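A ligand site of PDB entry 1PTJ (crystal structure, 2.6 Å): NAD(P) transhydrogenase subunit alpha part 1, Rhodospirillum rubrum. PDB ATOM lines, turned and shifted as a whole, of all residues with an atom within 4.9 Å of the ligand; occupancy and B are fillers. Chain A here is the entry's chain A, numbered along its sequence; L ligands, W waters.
The guanidinium group (NH2) of Arg 204 sits at hydrogen-bond distance from an oxygen (O12) of the ligand. The backbone NH of Ser 129 lies close to a sulfur (S1) of the ligand, at 3.7 Å. An oxygen (O4) of the ligand is in hydrogen-bond range of the backbone NH (N) of Leu 266 (3.3 Å). A nitrogen (N5) of the ligand lies close to the backbone NH of Val 203 (3.5 Å). N4 of the ligand lies close to OE1 of Gln 247, at 3.0 Å. O of Ile 128 sits at hydrogen-bond distance from N7 of the ligand. The backbone NH (N) of Ile 128 sits close to a sulfur (S1) of the ligand (3.8 Å). The side-chain carboxylate (OD2) of Asp 202 sits at hydrogen-bond distance from an oxygen (O5) of the ligand (2.5 Å). The backbone NH (N) of Gly 181 sits at hydrogen-bond distance from an oxygen (O5) of the ligand. N of Val 182 is in hydrogen-bond range of O8 of the ligand (3.0 Å).
O of Ser 129 is in hydrogen-bond range of NE2 of Gln 132 (3.2 Å). The guanidinium group (NH2) of Arg 204 is in hydrogen-bond range of the backbone carbonyl oxygen (O) of Val 180, at 3.5 Å. The side-chain carboxylate (OD2) of Asp 202 sits at hydrogen-bond distance from the backbone NH (N) of Val 180 (2.7 Å). OD1 of Asp 135 sits at hydrogen-bond distance from N of Ser 138 (3.0 Å). The backbone NH of Arg 204 lies within hydrogen-bond range of the side-chain carboxylate of Asp 202 (3.0 Å). The backbone carbonyl oxygen (O) of Gly 179 is in hydrogen-bond range of the side-chain hydroxyl (OG1) of Thr 264, 2.7 Å away.
The backbone carbonyl oxygen (O) of Arg 127 lies close to a sulfur (S1) of the ligand, 2.8 Å away. The backbone carbonyl oxygen (O) of Gly 234 sits close to an oxygen (O11) of the ligand, at 2.8 Å. Residues that only touch the ligand: Pro 126 (3.9 Å), Gln 132 (3.9 Å), Asp 135 (3.0 Å), Ser 138 (3.2 Å), Val 180 (3.7 Å), Thr 264 (3.2 Å), Ala 265 (3.3 Å), Ile 267 (3.8 Å), Pro 273 (3.7 Å) and Leu 275 (3.9 Å). Hydrophobic or aromatic side chains within 4 Å of the ligand: Val 203, Ala 265, Leu 266, Ile 267, Pro 273 and Leu 275. 21 residues have an atom within 4 Å of the ligand: Pro 126, Arg 127, Ile 128, Ser 129, Gln 132, Asp 135, Ser 138, Val 180, Gly 181, Val 182, Asp 202, Val 203, Arg 204, Gly 234, Gln 247, Thr 264, Ala 265, Leu 266, Ile 267, Pro 273 and Leu 275. Along chain A the residues within 4 Å of the ligand span positions 126 to 275.
Water W1 bridges O1 of the ligand (2.9 Å) and N of Ala 183 (3.2 Å).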
ATOM      1  N   PRO A 126     -34.993   2.280 -23.560  1.00  0.00           N
ATOM      2  CA  PRO A 126     -35.372   1.130 -22.735  1.00  0.00           C
ATOM      3  C   PRO A 126     -35.055  -0.219 -23.375  1.00  0.00           C
ATOM      4  O   PRO A 126     -35.032  -0.349 -24.601  1.00  0.00           O
ATOM      5  CB  PRO A 126     -36.868   1.348 -22.506  1.00  0.00           C
ATOM      6  CG  PRO A 126     -37.299   2.160 -23.692  1.00  0.00           C
ATOM      7  CD  PRO A 126     -36.166   3.138 -23.820  1.00  0.00           C
ATOM      8  N   ARG A 127     -34.804  -1.229 -22.535  1.00  0.00           N
ATOM      9  CA  ARG A 127     -34.487  -2.555 -23.028  1.00  0.00           C
ATOM     10  C   ARG A 127     -35.721  -3.372 -23.361  1.00  0.00           C
ATOM     11  O   ARG A 127     -35.793  -4.572 -23.060  1.00  0.00           O
ATOM     12  CB  ARG A 127     -33.634  -3.322 -22.014  1.00  0.00           C
ATOM     13  CG  ARG A 127     -32.147  -2.931 -22.006  1.00  0.00           C
ATOM     14  CD  ARG A 127     -31.291  -4.133 -21.569  1.00  0.00           C
ATOM     15  NE  ARG A 127     -29.896  -3.785 -21.298  1.00  0.00           N
ATOM     16  CZ  ARG A 127     -29.079  -3.185 -22.151  1.00  0.00           C
ATOM     17  NH1 ARG A 127     -29.507  -2.836 -23.362  1.00  0.00           N
ATOM     18  NH2 ARG A 127     -27.817  -2.931 -21.808  1.00  0.00           N
ATOM     19  N   ILE A 128     -36.714  -2.723 -23.971  1.00  0.00           N
ATOM     20  CA  ILE A 128     -37.933  -3.410 -24.366  1.00  0.00           C
ATOM     21  C   ILE A 128     -37.732  -4.030 -25.745  1.00  0.00           C
ATOM     22  O   ILE A 128     -37.045  -3.464 -26.599  1.00  0.00           O
ATOM     23  CB  ILE A 128     -39.142  -2.451 -24.379  1.00  0.00           C
ATOM     24  CG1 ILE A 128     -38.796  -1.183 -25.165  1.00  0.00           C
ATOM     25  CG2 ILE A 128     -39.558  -2.132 -22.941  1.00  0.00           C
ATOM     26  CD1 ILE A 128     -39.925  -0.185 -25.275  1.00  0.00           C
ATOM     27  N   SER A 129     -38.333  -5.204 -25.947  1.00  0.00           N
ATOM     28  CA  SER A 129     -38.202  -5.947 -27.194  1.00  0.00           C
ATOM     29  C   SER A 129     -38.703  -5.248 -28.465  1.00  0.00           C
ATOM     30  O   SER A 129     -38.357  -5.650 -29.567  1.00  0.00           O
ATOM     31  CB  SER A 129     -38.885  -7.303 -27.045  1.00  0.00           C
ATOM     32  OG  SER A 129     -38.547  -8.165 -28.120  1.00  0.00           O
ATOM     33  N   ALA A 131     -38.074  -2.133 -29.127  1.00  0.00           N
ATOM     34  CA  ALA A 131     -37.174  -1.019 -29.408  1.00  0.00           C
ATOM     35  C   ALA A 131     -35.854  -1.470 -29.977  1.00  0.00           C
ATOM     36  O   ALA A 131     -34.973  -0.645 -30.231  1.00  0.00           O
ATOM     37  CB  ALA A 131     -36.953  -0.202 -28.146  1.00  0.00           C
ATOM     38  N   GLN A 132     -35.686  -2.778 -30.187  1.00  0.00           N
ATOM     39  CA  GLN A 132     -34.432  -3.280 -30.730  1.00  0.00           C
ATOM     40  C   GLN A 132     -34.097  -2.527 -32.014  1.00  0.00           C
ATOM     41  O   GLN A 132     -32.938  -2.240 -32.270  1.00  0.00           O
ATOM     42  CB  GLN A 132     -34.513  -4.786 -31.003  1.00  0.00           C
ATOM     43  CG  GLN A 132     -34.776  -5.624 -29.752  1.00  0.00           C
ATOM     44  CD  GLN A 132     -34.757  -7.124 -30.028  1.00  0.00           C
ATOM     45  OE1 GLN A 132     -33.687  -7.728 -30.204  1.00  0.00           O
ATOM     46  NE2 GLN A 132     -35.939  -7.738 -30.075  1.00  0.00           N
ATOM     47  N   ASP A 135     -32.364   0.804 -30.994  1.00  0.00           N
ATOM     48  CA  ASP A 135     -31.280   0.736 -30.009  1.00  0.00           C
ATOM     49  C   ASP A 135     -29.903   0.987 -30.657  1.00  0.00           C
ATOM     50  O   ASP A 135     -29.418   0.140 -31.399  1.00  0.00           O
ATOM     51  CB  ASP A 135     -31.298  -0.663 -29.384  1.00  0.00           C
ATOM     52  CG  ASP A 135     -30.487  -0.739 -28.113  1.00  0.00           C
ATOM     53  OD1 ASP A 135     -29.330  -0.266 -28.089  1.00  0.00           O
ATOM     54  OD2 ASP A 135     -31.020  -1.309 -27.129  1.00  0.00           O
ATOM     55  N   SER A 138     -26.857  -1.428 -29.399  1.00  0.00           N
ATOM     56  CA  SER A 138     -26.851  -2.722 -30.101  1.00  0.00           C
ATOM     57  C   SER A 138     -26.300  -2.660 -31.534  1.00  0.00           C
ATOM     58  O   SER A 138     -25.387  -3.397 -31.889  1.00  0.00           O
ATOM     59  CB  SER A 138     -28.268  -3.298 -30.146  1.00  0.00           C
ATOM     60  OG  SER A 138     -28.830  -3.388 -28.854  1.00  0.00           O
ATOM     61  N   SER A 141     -22.672  -2.061 -31.035  1.00  0.00           N
ATOM     62  CA  SER A 141     -21.982  -3.145 -30.334  1.00  0.00           C
ATOM     63  C   SER A 141     -21.678  -4.222 -31.351  1.00  0.00           C
ATOM     64  O   SER A 141     -20.550  -4.691 -31.462  1.00  0.00           O
ATOM     65  CB  SER A 141     -22.871  -3.771 -29.267  1.00  0.00           C
ATOM     66  OG  SER A 141     -23.261  -2.840 -28.296  1.00  0.00           O
ATOM     67  N   GLY A 179     -17.541 -12.227 -21.997  1.00  0.00           N
ATOM     68  CA  GLY A 179     -18.723 -11.406 -22.155  1.00  0.00           C
ATOM     69  C   GLY A 179     -19.410 -11.717 -23.459  1.00  0.00           C
ATOM     70  O   GLY A 179     -18.980 -11.250 -24.514  1.00  0.00           O
ATOM     71  N   VAL A 180     -20.484 -12.518 -23.395  1.00  0.00           N
ATOM     72  CA  VAL A 180     -21.189 -12.900 -24.599  1.00  0.00           C
ATOM     73  C   VAL A 180     -22.492 -12.153 -24.852  1.00  0.00           C
ATOM     74  O   VAL A 180     -23.565 -12.741 -24.933  1.00  0.00           O
ATOM     75  CB  VAL A 180     -21.488 -14.413 -24.613  1.00  0.00           C
ATOM     76  CG1 VAL A 180     -21.795 -14.857 -26.027  1.00  0.00           C
ATOM     77  CG2 VAL A 180     -20.284 -15.194 -24.069  1.00  0.00           C
ATOM     78  N   GLY A 181     -22.385 -10.839 -24.960  1.00  0.00           N
ATOM     79  CA  GLY A 181     -23.552 -10.019 -25.247  1.00  0.00           C
ATOM     80  C   GLY A 181     -23.563  -9.814 -26.751  1.00  0.00           C
ATOM     81  O   GLY A 181     -23.098 -10.682 -27.503  1.00  0.00           O
ATOM     82  N   VAL A 182     -24.071  -8.666 -27.208  1.00  0.00           N
ATOM     83  CA  VAL A 182     -24.137  -8.382 -28.636  1.00  0.00           C
ATOM     84  C   VAL A 182     -22.752  -8.392 -29.244  1.00  0.00           C
ATOM     85  O   VAL A 182     -22.460  -9.212 -30.119  1.00  0.00           O
ATOM     86  CB  VAL A 182     -24.794  -7.029 -28.896  1.00  0.00           C
ATOM     87  CG1 VAL A 182     -24.695  -6.673 -30.353  1.00  0.00           C
ATOM     88  CG2 VAL A 182     -26.246  -7.081 -28.491  1.00  0.00           C
ATOM     89  N   ALA A 183     -21.888  -7.492 -28.779  1.00  0.00           N
ATOM     90  CA  ALA A 183     -20.532  -7.403 -29.286  1.00  0.00           C
ATOM     91  C   ALA A 183     -19.791  -8.735 -29.188  1.00  0.00           C
ATOM     92  O   ALA A 183     -19.040  -9.115 -30.113  1.00  0.00           O
ATOM     93  CB  ALA A 183     -19.774  -6.330 -28.518  1.00  0.00           C
ATOM     94  N   THR A 201     -17.300 -17.143 -22.143  1.00  0.00           N
ATOM     95  CA  THR A 201     -17.872 -17.202 -20.803  1.00  0.00           C
ATOM     96  C   THR A 201     -18.618 -15.904 -20.488  1.00  0.00           C
ATOM     97  O   THR A 201     -18.236 -14.828 -20.960  1.00  0.00           O
ATOM     98  CB  THR A 201     -16.778 -17.408 -19.730  1.00  0.00           C
ATOM     99  OG1 THR A 201     -17.396 -17.601 -18.449  1.00  0.00           O
ATOM    100  CG2 THR A 201     -15.872 -16.177 -19.663  1.00  0.00           C
ATOM    101  N   ASP A 202     -19.657 -16.021 -19.665  1.00  0.00           N
ATOM    102  CA  ASP A 202     -20.481 -14.882 -19.252  1.00  0.00           C
ATOM    103  C   ASP A 202     -21.149 -15.268 -17.923  1.00  0.00           C
ATOM    104  O   ASP A 202     -21.283 -16.456 -17.612  1.00  0.00           O
ATOM    105  CB  ASP A 202     -21.573 -14.598 -20.308  1.00  0.00           C
ATOM    106  CG  ASP A 202     -22.140 -13.189 -20.202  1.00  0.00           C
ATOM    107  OD1 ASP A 202     -22.635 -12.777 -19.126  1.00  0.00           O
ATOM    108  OD2 ASP A 202     -22.096 -12.472 -21.230  1.00  0.00           O
ATOM    109  N   VAL A 203     -21.560 -14.275 -17.142  1.00  0.00           N
ATOM    110  CA  VAL A 203     -22.234 -14.544 -15.896  1.00  0.00           C
ATOM    111  C   VAL A 203     -23.678 -14.926 -16.213  1.00  0.00           C
ATOM    112  O   VAL A 203     -24.190 -15.905 -15.673  1.00  0.00           O
ATOM    113  CB  VAL A 203     -22.198 -13.325 -14.956  1.00  0.00           C
ATOM    114  CG1 VAL A 203     -20.794 -13.128 -14.437  1.00  0.00           C
ATOM    115  CG2 VAL A 203     -22.663 -12.081 -15.684  1.00  0.00           C
ATOM    116  N   ARG A 204     -24.326 -14.182 -17.100  1.00  0.00           N
ATOM    117  CA  ARG A 204     -25.702 -14.495 -17.490  1.00  0.00           C
ATOM    118  C   ARG A 204     -25.753 -15.925 -18.028  1.00  0.00           C
ATOM    119  O   ARG A 204     -25.127 -16.229 -19.041  1.00  0.00           O
ATOM    120  CB  ARG A 204     -26.220 -13.528 -18.566  1.00  0.00           C
ATOM    121  CG  ARG A 204     -26.329 -12.070 -18.131  1.00  0.00           C
ATOM    122  CD  ARG A 204     -27.026 -11.189 -19.183  1.00  0.00           C
ATOM    123  NE  ARG A 204     -26.364 -11.220 -20.488  1.00  0.00           N
ATOM    124  CZ  ARG A 204     -26.713 -12.029 -21.490  1.00  0.00           C
ATOM    125  NH1 ARG A 204     -27.714 -12.888 -21.358  1.00  0.00           N
ATOM    126  NH2 ARG A 204     -26.034 -11.989 -22.632  1.00  0.00           N
ATOM    127  N   GLN A 210     -26.549 -19.927 -26.439  1.00  0.00           N
ATOM    128  CA  GLN A 210     -26.179 -19.151 -27.625  1.00  0.00           C
ATOM    129  C   GLN A 210     -24.759 -19.455 -28.117  1.00  0.00           C
ATOM    130  O   GLN A 210     -24.525 -19.620 -29.302  1.00  0.00           O
ATOM    131  CB  GLN A 210     -26.301 -17.643 -27.338  1.00  0.00           C
ATOM    132  CG  GLN A 210     -27.650 -17.211 -26.761  1.00  0.00           C
ATOM    133  CD  GLN A 210     -27.646 -15.809 -26.155  1.00  0.00           C
ATOM    134  OE1 GLN A 210     -27.739 -14.804 -26.872  1.00  0.00           O
ATOM    135  NE2 GLN A 210     -27.540 -15.732 -24.829  1.00  0.00           N
ATOM    136  N   GLY A 234     -32.385  -7.185 -18.211  1.00  0.00           N
ATOM    137  CA  GLY A 234     -31.753  -7.306 -19.513  1.00  0.00           C
ATOM    138  C   GLY A 234     -30.230  -7.304 -19.438  1.00  0.00           C
ATOM    139  O   GLY A 234     -29.560  -7.470 -20.462  1.00  0.00           O
ATOM    140  N   ALA A 236     -26.632  -7.305 -16.216  1.00  0.00           N
ATOM    141  CA  ALA A 236     -26.122  -7.806 -14.946  1.00  0.00           C
ATOM    142  C   ALA A 236     -25.590  -6.716 -14.018  1.00  0.00           C
ATOM    143  O   ALA A 236     -25.664  -5.513 -14.331  1.00  0.00           O
ATOM    144  CB  ALA A 236     -25.029  -8.835 -15.209  1.00  0.00           C
ATOM    145  N   MET A 239     -20.567  -8.938  -9.273  1.00  0.00           N
ATOM    146  CA  MET A 239     -20.694 -10.317  -8.815  1.00  0.00           C
ATOM    147  C   MET A 239     -20.055 -10.617  -7.457  1.00  0.00           C
ATOM    148  O   MET A 239     -20.396 -11.617  -6.820  1.00  0.00           O
ATOM    149  CB  MET A 239     -20.122 -11.259  -9.867  1.00  0.00           C
ATOM    150  CG  MET A 239     -20.994 -11.368 -11.086  1.00  0.00           C
ATOM    151  SD  MET A 239     -22.580 -12.039 -10.618  1.00  0.00           S
ATOM    152  CE  MET A 239     -22.266 -13.795 -10.775  1.00  0.00           C
ATOM    153  N   PHE A 243     -16.812 -14.480  -6.587  1.00  0.00           N
ATOM    154  CA  PHE A 243     -16.952 -15.004  -7.958  1.00  0.00           C
ATOM    155  C   PHE A 243     -15.708 -14.819  -8.823  1.00  0.00           C
ATOM    156  O   PHE A 243     -15.182 -15.780  -9.372  1.00  0.00           O
ATOM    157  CB  PHE A 243     -18.145 -14.345  -8.646  1.00  0.00           C
ATOM    158  CG  PHE A 243     -18.437 -14.900 -10.007  1.00  0.00           C
ATOM    159  CD1 PHE A 243     -18.791 -16.247 -10.171  1.00  0.00           C
ATOM    160  CD2 PHE A 243     -18.356 -14.100 -11.138  1.00  0.00           C
ATOM    161  CE1 PHE A 243     -19.069 -16.762 -11.424  1.00  0.00           C
ATOM    162  CE2 PHE A 243     -18.629 -14.602 -12.401  1.00  0.00           C
ATOM    163  CZ  PHE A 243     -18.992 -15.946 -12.547  1.00  0.00           C
ATOM    164  N   GLN A 247     -14.013 -17.535 -10.902  1.00  0.00           N
ATOM    165  CA  GLN A 247     -14.030 -17.347 -12.351  1.00  0.00           C
ATOM    166  C   GLN A 247     -12.684 -17.682 -12.973  1.00  0.00           C
ATOM    167  O   GLN A 247     -12.574 -18.599 -13.791  1.00  0.00           O
ATOM    168  CB  GLN A 247     -14.415 -15.904 -12.686  1.00  0.00           C
ATOM    169  CG  GLN A 247     -15.138 -15.738 -14.020  1.00  0.00           C
ATOM    170  CD  GLN A 247     -15.470 -14.291 -14.349  1.00  0.00           C
ATOM    171  OE1 GLN A 247     -16.336 -14.018 -15.187  1.00  0.00           O
ATOM    172  NE2 GLN A 247     -14.782 -13.361 -13.698  1.00  0.00           N
ATOM    173  N   THR A 264     -15.559  -7.876 -23.481  1.00  0.00           N
ATOM    174  CA  THR A 264     -16.711  -7.013 -23.763  1.00  0.00           C
ATOM    175  C   THR A 264     -17.644  -6.798 -22.568  1.00  0.00           C
ATOM    176  O   THR A 264     -18.747  -6.282 -22.745  1.00  0.00           O
ATOM    177  CB  THR A 264     -17.586  -7.606 -24.881  1.00  0.00           C
ATOM    178  OG1 THR A 264     -18.399  -8.648 -24.330  1.00  0.00           O
ATOM    179  CG2 THR A 264     -16.720  -8.203 -25.998  1.00  0.00           C
ATOM    180  N   ALA A 265     -17.203  -7.185 -21.370  1.00  0.00           N
ATOM    181  CA  ALA A 265     -18.021  -7.091 -20.158  1.00  0.00           C
ATOM    182  C   ALA A 265     -18.373  -5.693 -19.713  1.00  0.00           C
ATOM    183  O   ALA A 265     -17.510  -4.834 -19.613  1.00  0.00           O
ATOM    184  CB  ALA A 265     -17.360  -7.852 -19.032  1.00  0.00           C
ATOM    185  N   LEU A 266     -19.648  -5.481 -19.430  1.00  0.00           N
ATOM    186  CA  LEU A 266     -20.137  -4.181 -18.995  1.00  0.00           C
ATOM    187  C   LEU A 266     -21.172  -4.275 -17.874  1.00  0.00           C
ATOM    188  O   LEU A 266     -21.899  -5.261 -17.762  1.00  0.00           O
ATOM    189  CB  LEU A 266     -20.739  -3.456 -20.199  1.00  0.00           C
ATOM    190  CG  LEU A 266     -20.085  -2.149 -20.635  1.00  0.00           C
ATOM    191  CD1 LEU A 266     -18.579  -2.356 -20.779  1.00  0.00           C
ATOM    192  CD2 LEU A 266     -20.706  -1.670 -21.941  1.00  0.00           C
ATOM    193  N   ILE A 267     -21.220  -3.248 -17.044  1.00  0.00           N
ATOM    194  CA  ILE A 267     -22.162  -3.193 -15.931  1.00  0.00           C
ATOM    195  C   ILE A 267     -22.560  -1.732 -15.690  1.00  0.00           C
ATOM    196  O   ILE A 267     -21.753  -0.939 -15.190  1.00  0.00           O
ATOM    197  CB  ILE A 267     -21.555  -3.763 -14.624  1.00  0.00           C
ATOM    198  CG1 ILE A 267     -21.415  -5.283 -14.727  1.00  0.00           C
ATOM    199  CG2 ILE A 267     -22.445  -3.424 -13.439  1.00  0.00           C
ATOM    200  CD1 ILE A 267     -20.776  -5.932 -13.510  1.00  0.00           C
ATOM    201  N   PRO A 273     -16.045  -4.370 -15.322  1.00  0.00           N
ATOM    202  CA  PRO A 273     -15.473  -5.479 -14.570  1.00  0.00           C
ATOM    203  C   PRO A 273     -14.144  -6.061 -15.064  1.00  0.00           C
ATOM    204  O   PRO A 273     -14.047  -6.581 -16.178  1.00  0.00           O
ATOM    205  CB  PRO A 273     -16.590  -6.514 -14.577  1.00  0.00           C
ATOM    206  CG  PRO A 273     -17.323  -6.215 -15.826  1.00  0.00           C
ATOM    207  CD  PRO A 273     -17.378  -4.714 -15.834  1.00  0.00           C
ATOM    208  N   LEU A 275     -11.522  -8.593 -15.785  1.00  0.00           N
ATOM    209  CA  LEU A 275     -11.585 -10.027 -15.997  1.00  0.00           C
ATOM    210  C   LEU A 275     -10.211 -10.630 -16.281  1.00  0.00           C
ATOM    211  O   LEU A 275     -10.021 -11.845 -16.190  1.00  0.00           O
ATOM    212  CB  LEU A 275     -12.512 -10.328 -17.160  1.00  0.00           C
ATOM    213  CG  LEU A 275     -13.879  -9.662 -17.027  1.00  0.00           C
ATOM    214  CD1 LEU A 275     -14.639  -9.763 -18.345  1.00  0.00           C
ATOM    215  CD2 LEU A 275     -14.642 -10.328 -15.886  1.00  0.00           C
HETATM  216  P1  LIG L   1     -23.533  -5.147 -22.245  1.00  0.00           P
HETATM  217  O1  LIG L   1     -22.724  -4.786 -23.436  1.00  0.00           O
HETATM  218  O2  LIG L   1     -23.588  -4.034 -21.266  1.00  0.00           O
HETATM  219  O3  LIG L   1     -22.937  -6.459 -21.553  1.00  0.00           O
HETATM  220  C1  LIG L   1     -21.762  -7.138 -22.054  1.00  0.00           C
HETATM  221  C2  LIG L   1     -21.705  -8.529 -21.447  1.00  0.00           C
HETATM  222  O4  LIG L   1     -21.024  -8.404 -20.175  1.00  0.00           O
HETATM  223  C3  LIG L   1     -23.037  -9.209 -21.056  1.00  0.00           C
HETATM  224  O5  LIG L   1     -23.400 -10.377 -21.757  1.00  0.00           O
HETATM  225  C4  LIG L   1     -22.898  -9.409 -19.549  1.00  0.00           C
HETATM  226  O6  LIG L   1     -23.708 -10.414 -18.987  1.00  0.00           O
HETATM  227  C5  LIG L   1     -21.390  -9.583 -19.477  1.00  0.00           C
HETATM  228  N1  LIG L   1     -20.749  -9.466 -18.135  1.00  0.00           N
HETATM  229  C6  LIG L   1     -20.839  -8.438 -17.213  1.00  0.00           C
HETATM  230  N2  LIG L   1     -20.112  -8.643 -16.092  1.00  0.00           N
HETATM  231  C7  LIG L   1     -19.531  -9.867 -16.310  1.00  0.00           C
HETATM  232  C8  LIG L   1     -18.636 -10.677 -15.521  1.00  0.00           C
HETATM  233  N3  LIG L   1     -18.183 -10.326 -14.316  1.00  0.00           N
HETATM  234  N4  LIG L   1     -18.224 -11.914 -16.061  1.00  0.00           N
HETATM  235  C9  LIG L   1     -18.669 -12.318 -17.326  1.00  0.00           C
HETATM  236  N5  LIG L   1     -19.491 -11.627 -18.110  1.00  0.00           N
HETATM  237  C10 LIG L   1     -19.904 -10.404 -17.568  1.00  0.00           C
HETATM  238  O7  LIG L   1     -24.889  -5.844 -22.612  1.00  0.00           O
HETATM  239  P2  LIG L   1     -25.467  -6.159 -23.981  1.00  0.00           P
HETATM  240  O8  LIG L   1     -24.520  -7.006 -24.754  1.00  0.00           O
HETATM  241  O9  LIG L   1     -25.699  -4.890 -24.720  1.00  0.00           O
HETATM  242  O10 LIG L   1     -26.760  -6.874 -23.794  1.00  0.00           O
HETATM  243  C11 LIG L   1     -26.946  -8.188 -23.385  1.00  0.00           C
HETATM  244  C12 LIG L   1     -28.065  -8.789 -23.239  1.00  0.00           C
HETATM  245  O11 LIG L   1     -29.103  -7.756 -23.233  1.00  0.00           O
HETATM  246  C13 LIG L   1     -28.260  -9.692 -24.468  1.00  0.00           C
HETATM  247  O12 LIG L   1     -28.651 -10.996 -24.025  1.00  0.00           O
HETATM  248  C14 LIG L   1     -29.323  -8.944 -25.310  1.00  0.00           C
HETATM  249  O13 LIG L   1     -30.131  -9.571 -25.780  1.00  0.00           O
HETATM  250  C15 LIG L   1     -29.979  -7.939 -24.378  1.00  0.00           C
HETATM  251  N6  LIG L   1     -30.282  -6.664 -24.974  1.00  0.00           N
HETATM  252  C16 LIG L   1     -31.650  -6.339 -25.097  1.00  0.00           C
HETATM  253  C17 LIG L   1     -32.009  -5.116 -25.684  1.00  0.00           C
HETATM  254  C18 LIG L   1     -33.457  -4.542 -25.921  1.00  0.00           C
HETATM  255  S1  LIG L   1     -34.683  -5.497 -25.480  1.00  0.00           S
HETATM  256  N7  LIG L   1     -33.749  -3.453 -26.653  1.00  0.00           N
HETATM  257  C19 LIG L   1     -30.987  -4.178 -26.168  1.00  0.00           C
HETATM  258  C20 LIG L   1     -29.633  -4.572 -26.024  1.00  0.00           C
HETATM  259  C21 LIG L   1     -29.192  -5.766 -25.451  1.00  0.00           C
HETATM  260  O   HOH W   1     -21.854  -6.203 -25.840  1.00  0.00           O
